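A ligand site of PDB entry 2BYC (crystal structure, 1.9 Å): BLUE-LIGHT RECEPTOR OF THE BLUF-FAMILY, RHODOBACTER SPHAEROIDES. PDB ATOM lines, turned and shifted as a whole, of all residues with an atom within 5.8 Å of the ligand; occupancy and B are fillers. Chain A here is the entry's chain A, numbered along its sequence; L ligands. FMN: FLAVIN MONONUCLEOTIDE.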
ATOM      1  N   TYR A  10     -20.681 -24.709  18.193  1.00  0.00           N
ATOM      2  CA  TYR A  10     -22.027 -24.248  18.392  1.00  0.00           C
ATOM      3  C   TYR A  10     -22.955 -25.456  18.246  1.00  0.00           C
ATOM      4  O   TYR A  10     -22.582 -26.491  17.737  1.00  0.00           O
ATOM      5  CB  TYR A  10     -22.379 -23.101  17.371  1.00  0.00           C
ATOM      6  CG  TYR A  10     -22.554 -23.646  15.984  1.00  0.00           C
ATOM      7  CD1 TYR A  10     -23.690 -24.355  15.670  1.00  0.00           C
ATOM      8  CD2 TYR A  10     -21.588 -23.431  14.992  1.00  0.00           C
ATOM      9  CE1 TYR A  10     -23.847 -24.905  14.428  1.00  0.00           C
ATOM     10  CE2 TYR A  10     -21.751 -23.968  13.715  1.00  0.00           C
ATOM     11  CZ  TYR A  10     -22.895 -24.673  13.448  1.00  0.00           C
ATOM     12  OH  TYR A  10     -23.137 -25.256  12.250  1.00  0.00           O
ATOM     13  N   SER A  12     -27.019 -26.370  17.151  1.00  0.00           N
ATOM     14  CA  SER A  12     -28.244 -25.859  16.509  1.00  0.00           C
ATOM     15  C   SER A  12     -29.236 -26.941  16.391  1.00  0.00           C
ATOM     16  O   SER A  12     -28.888 -28.111  16.517  1.00  0.00           O
ATOM     17  CB  SER A  12     -28.005 -25.320  15.107  1.00  0.00           C
ATOM     18  OG  SER A  12     -27.533 -26.308  14.260  1.00  0.00           O
ATOM     19  N   GLN A  25     -25.449 -31.487   0.265  1.00  0.00           N
ATOM     20  CA  GLN A  25     -25.132 -30.134  -0.211  1.00  0.00           C
ATOM     21  C   GLN A  25     -24.278 -29.388   0.820  1.00  0.00           C
ATOM     22  O   GLN A  25     -23.413 -28.617   0.477  1.00  0.00           O
ATOM     23  CB  GLN A  25     -26.405 -29.315  -0.424  1.00  0.00           C
ATOM     24  CG  GLN A  25     -27.399 -29.848  -1.497  1.00  0.00           C
ATOM     25  CD  GLN A  25     -28.846 -29.153  -1.524  1.00  0.00           C
ATOM     26  OE1 GLN A  25     -29.022 -28.058  -2.126  1.00  0.00           O
ATOM     27  NE2 GLN A  25     -29.870 -29.843  -0.986  1.00  0.00           N
ATOM     28  N   ILE A  26     -24.535 -29.596   2.102  1.00  0.00           N
ATOM     29  CA  ILE A  26     -23.730 -28.936   3.114  1.00  0.00           C
ATOM     30  C   ILE A  26     -22.337 -29.443   3.031  1.00  0.00           C
ATOM     31  O   ILE A  26     -21.425 -28.684   3.220  1.00  0.00           O
ATOM     32  CB  ILE A  26     -24.279 -29.148   4.517  1.00  0.00           C
ATOM     33  CG1 ILE A  26     -25.608 -28.377   4.643  1.00  0.00           C
ATOM     34  CG2 ILE A  26     -23.206 -28.766   5.492  1.00  0.00           C
ATOM     35  CD1 ILE A  26     -26.381 -28.644   5.881  1.00  0.00           C
ATOM     36  N   ALA A  29     -20.555 -28.067  -0.236  1.00  0.00           N
ATOM     37  CA  ALA A  29     -20.265 -26.678   0.009  1.00  0.00           C
ATOM     38  C   ALA A  29     -19.106 -26.418   0.915  1.00  0.00           C
ATOM     39  O   ALA A  29     -18.270 -25.615   0.612  1.00  0.00           O
ATOM     40  CB  ALA A  29     -21.496 -25.971   0.569  1.00  0.00           C
ATOM     41  N   SER A  30     -19.058 -27.145   2.049  1.00  0.00           N
ATOM     42  CA  SER A  30     -18.135 -26.882   3.100  1.00  0.00           C
ATOM     43  C   SER A  30     -16.752 -27.402   2.746  1.00  0.00           C
ATOM     44  O   SER A  30     -15.751 -26.779   3.057  1.00  0.00           O
ATOM     45  CB  SER A  30     -18.627 -27.558   4.363  1.00  0.00           C
ATOM     46  OG  SER A  30     -18.451 -28.908   4.155  1.00  0.00           O
ATOM     47  N   ARG A  31     -16.680 -28.537   2.064  1.00  0.00           N
ATOM     48  CA  ARG A  31     -15.402 -29.053   1.685  1.00  0.00           C
ATOM     49  C   ARG A  31     -14.626 -28.001   0.829  1.00  0.00           C
ATOM     50  O   ARG A  31     -13.406 -27.774   1.025  1.00  0.00           O
ATOM     51  CB  ARG A  31     -15.571 -30.407   0.963  1.00  0.00           C
ATOM     52  CG  ARG A  31     -14.253 -31.112   0.710  1.00  0.00           C
ATOM     53  CD  ARG A  31     -14.317 -32.228  -0.326  1.00  0.00           C
ATOM     54  NE  ARG A  31     -12.988 -32.861  -0.387  1.00  0.00           N
ATOM     55  CZ  ARG A  31     -12.656 -33.993  -1.036  1.00  0.00           C
ATOM     56  NH1 ARG A  31     -13.550 -34.695  -1.767  1.00  0.00           N
ATOM     57  NH2 ARG A  31     -11.399 -34.422  -0.987  1.00  0.00           N
ATOM     58  N   ARG A  33     -15.272 -24.445   0.477  1.00  0.00           N
ATOM     59  CA  ARG A  33     -15.141 -23.242   1.307  1.00  0.00           C
ATOM     60  C   ARG A  33     -14.129 -23.417   2.421  1.00  0.00           C
ATOM     61  O   ARG A  33     -13.181 -22.629   2.571  1.00  0.00           O
ATOM     62  CB  ARG A  33     -16.516 -22.919   1.920  1.00  0.00           C
ATOM     63  CG  ARG A  33     -16.639 -21.659   2.752  1.00  0.00           C
ATOM     64  CD  ARG A  33     -16.958 -20.492   1.842  1.00  0.00           C
ATOM     65  NE  ARG A  33     -18.369 -20.103   1.727  1.00  0.00           N
ATOM     66  CZ  ARG A  33     -19.329 -20.736   1.070  1.00  0.00           C
ATOM     67  NH1 ARG A  33     -19.125 -21.884   0.495  1.00  0.00           N
ATOM     68  NH2 ARG A  33     -20.529 -20.225   1.046  1.00  0.00           N
ATOM     69  N   ASN A  34     -14.289 -24.458   3.220  1.00  0.00           N
ATOM     70  CA  ASN A  34     -13.333 -24.600   4.339  1.00  0.00           C
ATOM     71  C   ASN A  34     -11.875 -24.720   3.873  1.00  0.00           C
ATOM     72  O   ASN A  34     -10.929 -24.168   4.454  1.00  0.00           O
ATOM     73  CB  ASN A  34     -13.714 -25.784   5.248  1.00  0.00           C
ATOM     74  CG  ASN A  34     -14.985 -25.556   5.960  1.00  0.00           C
ATOM     75  OD1 ASN A  34     -15.622 -24.536   5.783  1.00  0.00           O
ATOM     76  ND2 ASN A  34     -15.399 -26.491   6.761  1.00  0.00           N
ATOM     77  N   ILE A  39     -10.330 -23.400   7.080  1.00  0.00           N
ATOM     78  CA  ILE A  39     -11.073 -24.033   8.177  1.00  0.00           C
ATOM     79  C   ILE A  39     -11.001 -25.557   8.209  1.00  0.00           C
ATOM     80  O   ILE A  39     -10.942 -26.162   7.184  1.00  0.00           O
ATOM     81  CB  ILE A  39     -12.576 -23.607   8.113  1.00  0.00           C
ATOM     82  CG1 ILE A  39     -12.649 -22.092   8.127  1.00  0.00           C
ATOM     83  CG2 ILE A  39     -13.355 -24.196   9.232  1.00  0.00           C
ATOM     84  CD1 ILE A  39     -12.254 -21.552   9.455  1.00  0.00           C
ATOM     85  N   LEU A  43     -18.667 -31.945  12.060  1.00  0.00           N
ATOM     86  CA  LEU A  43     -20.062 -31.693  12.239  1.00  0.00           C
ATOM     87  C   LEU A  43     -20.741 -32.919  12.755  1.00  0.00           C
ATOM     88  O   LEU A  43     -20.656 -34.005  12.161  1.00  0.00           O
ATOM     89  CB  LEU A  43     -20.596 -31.384  10.909  1.00  0.00           C
ATOM     90  CG  LEU A  43     -22.083 -31.103  10.653  1.00  0.00           C
ATOM     91  CD1 LEU A  43     -22.567 -29.944  11.484  1.00  0.00           C
ATOM     92  CD2 LEU A  43     -22.346 -30.933   9.160  1.00  0.00           C
ATOM     93  N   PHE A  50     -27.462 -30.247  15.396  1.00  0.00           N
ATOM     94  CA  PHE A  50     -26.045 -30.343  14.878  1.00  0.00           C
ATOM     95  C   PHE A  50     -25.214 -29.765  15.971  1.00  0.00           C
ATOM     96  O   PHE A  50     -25.648 -28.837  16.679  1.00  0.00           O
ATOM     97  CB  PHE A  50     -25.901 -29.351  13.738  1.00  0.00           C
ATOM     98  CG  PHE A  50     -26.545 -29.765  12.453  1.00  0.00           C
ATOM     99  CD1 PHE A  50     -27.535 -28.974  11.852  1.00  0.00           C
ATOM    100  CD2 PHE A  50     -26.162 -30.917  11.800  1.00  0.00           C
ATOM    101  CE1 PHE A  50     -28.087 -29.351  10.586  1.00  0.00           C
ATOM    102  CE2 PHE A  50     -26.729 -31.287  10.592  1.00  0.00           C
ATOM    103  CZ  PHE A  50     -27.691 -30.463   9.980  1.00  0.00           C
ATOM    104  N   GLN A  52     -21.371 -28.348  15.725  1.00  0.00           N
ATOM    105  CA  GLN A  52     -20.279 -28.108  14.788  1.00  0.00           C
ATOM    106  C   GLN A  52     -19.080 -27.460  15.478  1.00  0.00           C
ATOM    107  O   GLN A  52     -19.260 -26.575  16.283  1.00  0.00           O
ATOM    108  CB  GLN A  52     -20.742 -27.327  13.538  1.00  0.00           C
ATOM    109  CG  GLN A  52     -19.649 -27.356  12.529  1.00  0.00           C
ATOM    110  CD  GLN A  52     -20.013 -26.640  11.268  1.00  0.00           C
ATOM    111  OE1 GLN A  52     -20.759 -25.666  11.256  1.00  0.00           O
ATOM    112  NE2 GLN A  52     -19.479 -27.129  10.189  1.00  0.00           N
ATOM    113  N   ILE A  54     -15.481 -25.705  14.329  1.00  0.00           N
ATOM    114  CA  ILE A  54     -14.639 -25.259  13.187  1.00  0.00           C
ATOM    115  C   ILE A  54     -13.466 -24.602  13.778  1.00  0.00           C
ATOM    116  O   ILE A  54     -13.582 -23.955  14.831  1.00  0.00           O
ATOM    117  CB  ILE A  54     -15.362 -24.185  12.332  1.00  0.00           C
ATOM    118  CG1 ILE A  54     -15.855 -23.055  13.238  1.00  0.00           C
ATOM    119  CG2 ILE A  54     -16.481 -24.821  11.471  1.00  0.00           C
ATOM    120  CD1 ILE A  54     -16.603 -21.970  12.573  1.00  0.00           C
ATOM    121  N   LEU A  64     -17.189 -17.503   8.620  1.00  0.00           N
ATOM    122  CA  LEU A  64     -17.875 -18.712   8.357  1.00  0.00           C
ATOM    123  C   LEU A  64     -19.065 -18.779   9.242  1.00  0.00           C
ATOM    124  O   LEU A  64     -20.147 -19.123   8.799  1.00  0.00           O
ATOM    125  CB  LEU A  64     -16.928 -19.904   8.556  1.00  0.00           C
ATOM    126  CG  LEU A  64     -17.595 -21.209   8.068  1.00  0.00           C
ATOM    127  CD1 LEU A  64     -18.170 -21.242   6.562  1.00  0.00           C
ATOM    128  CD2 LEU A  64     -16.763 -22.443   8.357  1.00  0.00           C
ATOM    129  N   LEU A  67     -21.920 -16.891   7.962  1.00  0.00           N
ATOM    130  CA  LEU A  67     -22.624 -17.550   6.848  1.00  0.00           C
ATOM    131  C   LEU A  67     -23.485 -18.685   7.321  1.00  0.00           C
ATOM    132  O   LEU A  67     -24.646 -18.797   6.965  1.00  0.00           O
ATOM    133  CB  LEU A  67     -21.584 -18.099   5.892  1.00  0.00           C
ATOM    134  CG  LEU A  67     -21.327 -17.067   4.818  1.00  0.00           C
ATOM    135  CD1 LEU A  67     -20.014 -17.345   4.072  1.00  0.00           C
ATOM    136  CD2 LEU A  67     -22.612 -16.983   3.878  1.00  0.00           C
ATOM    137  N   ILE A  68     -22.909 -19.542   8.129  1.00  0.00           N
ATOM    138  CA  ILE A  68     -23.587 -20.695   8.663  1.00  0.00           C
ATOM    139  C   ILE A  68     -24.832 -20.296   9.515  1.00  0.00           C
ATOM    140  O   ILE A  68     -25.839 -21.003   9.562  1.00  0.00           O
ATOM    141  CB  ILE A  68     -22.587 -21.536   9.490  1.00  0.00           C
ATOM    142  CG1 ILE A  68     -21.435 -22.135   8.640  1.00  0.00           C
ATOM    143  CG2 ILE A  68     -23.266 -22.657  10.099  1.00  0.00           C
ATOM    144  CD1 ILE A  68     -20.414 -22.777   9.532  1.00  0.00           C
ATOM    145  N   ASP A  71     -27.928 -19.689   7.599  1.00  0.00           N
ATOM    146  CA  ASP A  71     -28.487 -20.883   6.957  1.00  0.00           C
ATOM    147  C   ASP A  71     -29.835 -21.384   7.502  1.00  0.00           C
ATOM    148  O   ASP A  71     -30.027 -21.644   8.686  1.00  0.00           O
ATOM    149  CB  ASP A  71     -27.414 -21.955   6.854  1.00  0.00           C
ATOM    150  CG  ASP A  71     -27.804 -23.078   5.910  1.00  0.00           C
ATOM    151  OD1 ASP A  71     -28.959 -23.528   5.955  1.00  0.00           O
ATOM    152  OD2 ASP A  71     -26.971 -23.533   5.113  1.00  0.00           O
ATOM    153  N   ARG A  73     -31.270 -24.170   7.319  1.00  0.00           N
ATOM    154  CA  ARG A  73     -31.428 -25.596   7.555  1.00  0.00           C
ATOM    155  C   ARG A  73     -31.158 -25.941   9.001  1.00  0.00           C
ATOM    156  O   ARG A  73     -31.098 -27.136   9.364  1.00  0.00           O
ATOM    157  CB  ARG A  73     -30.558 -26.405   6.583  1.00  0.00           C
ATOM    158  CG  ARG A  73     -30.962 -26.193   5.082  1.00  0.00           C
ATOM    159  CD  ARG A  73     -29.965 -26.815   4.160  1.00  0.00           C
ATOM    160  NE  ARG A  73     -28.861 -25.899   3.943  1.00  0.00           N
ATOM    161  CZ  ARG A  73     -27.850 -26.130   3.128  1.00  0.00           C
ATOM    162  NH1 ARG A  73     -27.771 -27.260   2.406  1.00  0.00           N
ATOM    163  NH2 ARG A  73     -26.863 -25.239   3.083  1.00  0.00           N
ATOM    164  N   HIS A  74     -31.000 -24.919   9.842  1.00  0.00           N
ATOM    165  CA  HIS A  74     -30.935 -25.129  11.303  1.00  0.00           C
ATOM    166  C   HIS A  74     -31.403 -23.895  12.030  1.00  0.00           C
ATOM    167  O   HIS A  74     -31.382 -22.858  11.443  1.00  0.00           O
ATOM    168  CB  HIS A  74     -29.531 -25.570  11.816  1.00  0.00           C
ATOM    169  CG  HIS A  74     -28.405 -24.617  11.531  1.00  0.00           C
ATOM    170  ND1 HIS A  74     -27.150 -24.776  12.095  1.00  0.00           N
ATOM    171  CD2 HIS A  74     -28.302 -23.517  10.737  1.00  0.00           C
ATOM    172  CE1 HIS A  74     -26.332 -23.837  11.654  1.00  0.00           C
ATOM    173  NE2 HIS A  74     -27.001 -23.057  10.833  1.00  0.00           N
ATOM    174  N   SER A  94     -11.350 -30.823   6.521  1.00  0.00           N
ATOM    175  CA  SER A  94     -12.060 -29.650   6.112  1.00  0.00           C
ATOM    176  C   SER A  94     -13.437 -29.556   6.804  1.00  0.00           C
ATOM    177  O   SER A  94     -13.754 -28.513   7.320  1.00  0.00           O
ATOM    178  CB  SER A  94     -12.210 -29.717   4.591  1.00  0.00           C
ATOM    179  OG  SER A  94     -12.656 -28.491   4.077  1.00  0.00           O
ATOM    180  N   MET A  95     -14.184 -30.660   6.807  1.00  0.00           N
ATOM    181  CA  MET A  95     -15.409 -30.845   7.633  1.00  0.00           C
ATOM    182  C   MET A  95     -15.562 -32.359   7.579  1.00  0.00           C
ATOM    183  O   MET A  95     -15.552 -32.919   6.542  1.00  0.00           O
ATOM    184  CB  MET A  95     -16.598 -30.053   7.062  1.00  0.00           C
ATOM    185  CG  MET A  95     -17.802 -29.802   8.001  1.00  0.00           C
ATOM    186  SD  MET A  95     -17.230 -29.738   9.669  1.00  0.00           S
ATOM    187  CE  MET A  95     -16.242 -28.210   9.697  1.00  0.00           C
HETATM  188  N1  FMN L   1     -20.646 -24.206   4.829  1.00  0.00           N
HETATM  189  C2  FMN L   1     -19.273 -24.186   4.802  1.00  0.00           C
HETATM  190  O2  FMN L   1     -18.660 -23.659   3.834  1.00  0.00           O
HETATM  191  N3  FMN L   1     -18.537 -24.739   5.804  1.00  0.00           N
HETATM  192  C4  FMN L   1     -19.221 -25.339   6.804  1.00  0.00           C
HETATM  193  O4  FMN L   1     -18.596 -25.768   7.719  1.00  0.00           O
HETATM  194  C4A FMN L   1     -20.615 -25.371   6.849  1.00  0.00           C
HETATM  195  N5  FMN L   1     -21.266 -25.984   7.901  1.00  0.00           N
HETATM  196  C5A FMN L   1     -22.668 -25.956   7.998  1.00  0.00           C
HETATM  197  C6  FMN L   1     -23.325 -26.540   9.062  1.00  0.00           C
HETATM  198  C7  FMN L   1     -24.721 -26.589   9.164  1.00  0.00           C
HETATM  199  C7M FMN L   1     -25.403 -27.098  10.430  1.00  0.00           C
HETATM  200  C8  FMN L   1     -25.457 -25.996   8.155  1.00  0.00           C
HETATM  201  C8M FMN L   1     -26.971 -25.942   8.198  1.00  0.00           C
HETATM  202  C9  FMN L   1     -24.806 -25.399   7.074  1.00  0.00           C
HETATM  203  C9A FMN L   1     -23.384 -25.375   7.007  1.00  0.00           C
HETATM  204  N10 FMN L   1     -22.711 -24.790   5.908  1.00  0.00           N
HETATM  205  C10 FMN L   1     -21.324 -24.778   5.858  1.00  0.00           C
HETATM  206  C1' FMN L   1     -23.416 -24.432   4.645  1.00  0.00           C
HETATM  207  C2' FMN L   1     -23.240 -22.930   4.595  1.00  0.00           C
HETATM  208  O2' FMN L   1     -24.313 -22.491   5.375  1.00  0.00           O
HETATM  209  C3' FMN L   1     -23.255 -22.300   3.184  1.00  0.00           C
HETATM  210  O3' FMN L   1     -24.562 -22.333   2.698  1.00  0.00           O
HETATM  211  C4' FMN L   1     -22.340 -22.921   2.139  1.00  0.00           C
HETATM  212  O4' FMN L   1     -20.937 -22.703   2.385  1.00  0.00           O
HETATM  213  C5' FMN L   1     -22.646 -22.294   0.781  1.00  0.00           C
HETATM  214  O5' FMN L   1     -23.446 -23.065  -0.128  1.00  0.00           O
HETATM  215  P   FMN L   1     -23.403 -22.483  -1.624  1.00  0.00           P
HETATM  216  O1P FMN L   1     -24.153 -23.413  -2.602  1.00  0.00           O
HETATM  217  O2P FMN L   1     -24.093 -21.135  -1.524  1.00  0.00           O
HETATM  218  O3P FMN L   1     -21.920 -22.393  -1.886  1.00  0.00           O
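The guanidinium group of Arg 73 lies within salt-bridge range of the side-chain carboxylate of Asp 71, at 2.7 Å.
O of Asn 34 sits at hydrogen-bond distance from N of Ile 39.
The side-chain amide oxygen of Gln 52 lies within hydrogen-bond range of the side-chain hydroxyl of Tyr 10 (2.6 Å).
NE2 of Gln 52 lies close to SD of Met 95, 3.5 Å away.
The side-chain hydroxyl of Ser 30 is in hydrogen-bond range of the backbone carbonyl oxygen of Ile 26, at 3.1 Å.
The backbone carbonyl oxygen (O) of Ser 12 sits at hydrogen-bond distance from the backbone NH (N) of Phe 50, at 2.8 Å.
NE2 of His 74 is in hydrogen-bond range of O of Ile 68 (2.7 Å).
The side-chain sulfur (SD) of Met 95 lies within hydrogen-bond range of the backbone NH (N) of Leu 43 (3.6 Å).
Merely in contact with the ligand: Tyr 10, Ile 26, Ala 29, Ser 30, Phe 50, Leu 64, Ile 68, Arg 73, His 74 and Met 95.
Within 4 Å of the ligand: Tyr 10, Ile 26, Ala 29, Ser 30, Arg 33, Asn 34, Phe 50, Gln 52, Leu 64, Ile 68, Asp 71, Arg 73, His 74 and Met 95.
The nearest printed residue that does not touch the ligand is Leu 67 (4.04 Å).
An oxygen (O3P) of the ligand lies within salt-bridge range of the guanidinium group of Arg 33, at 3.7 Å.
O2' of the ligand is in hydrogen-bond range of OD2 of Asp 71 (2.9 Å).
A nitrogen (N3) of the ligand sits at hydrogen-bond distance from the side-chain amide oxygen (OD1) of Asn 34 (2.9 Å).
NE2 of Gln 52 sits at hydrogen-bond distance from O4 of the ligand.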
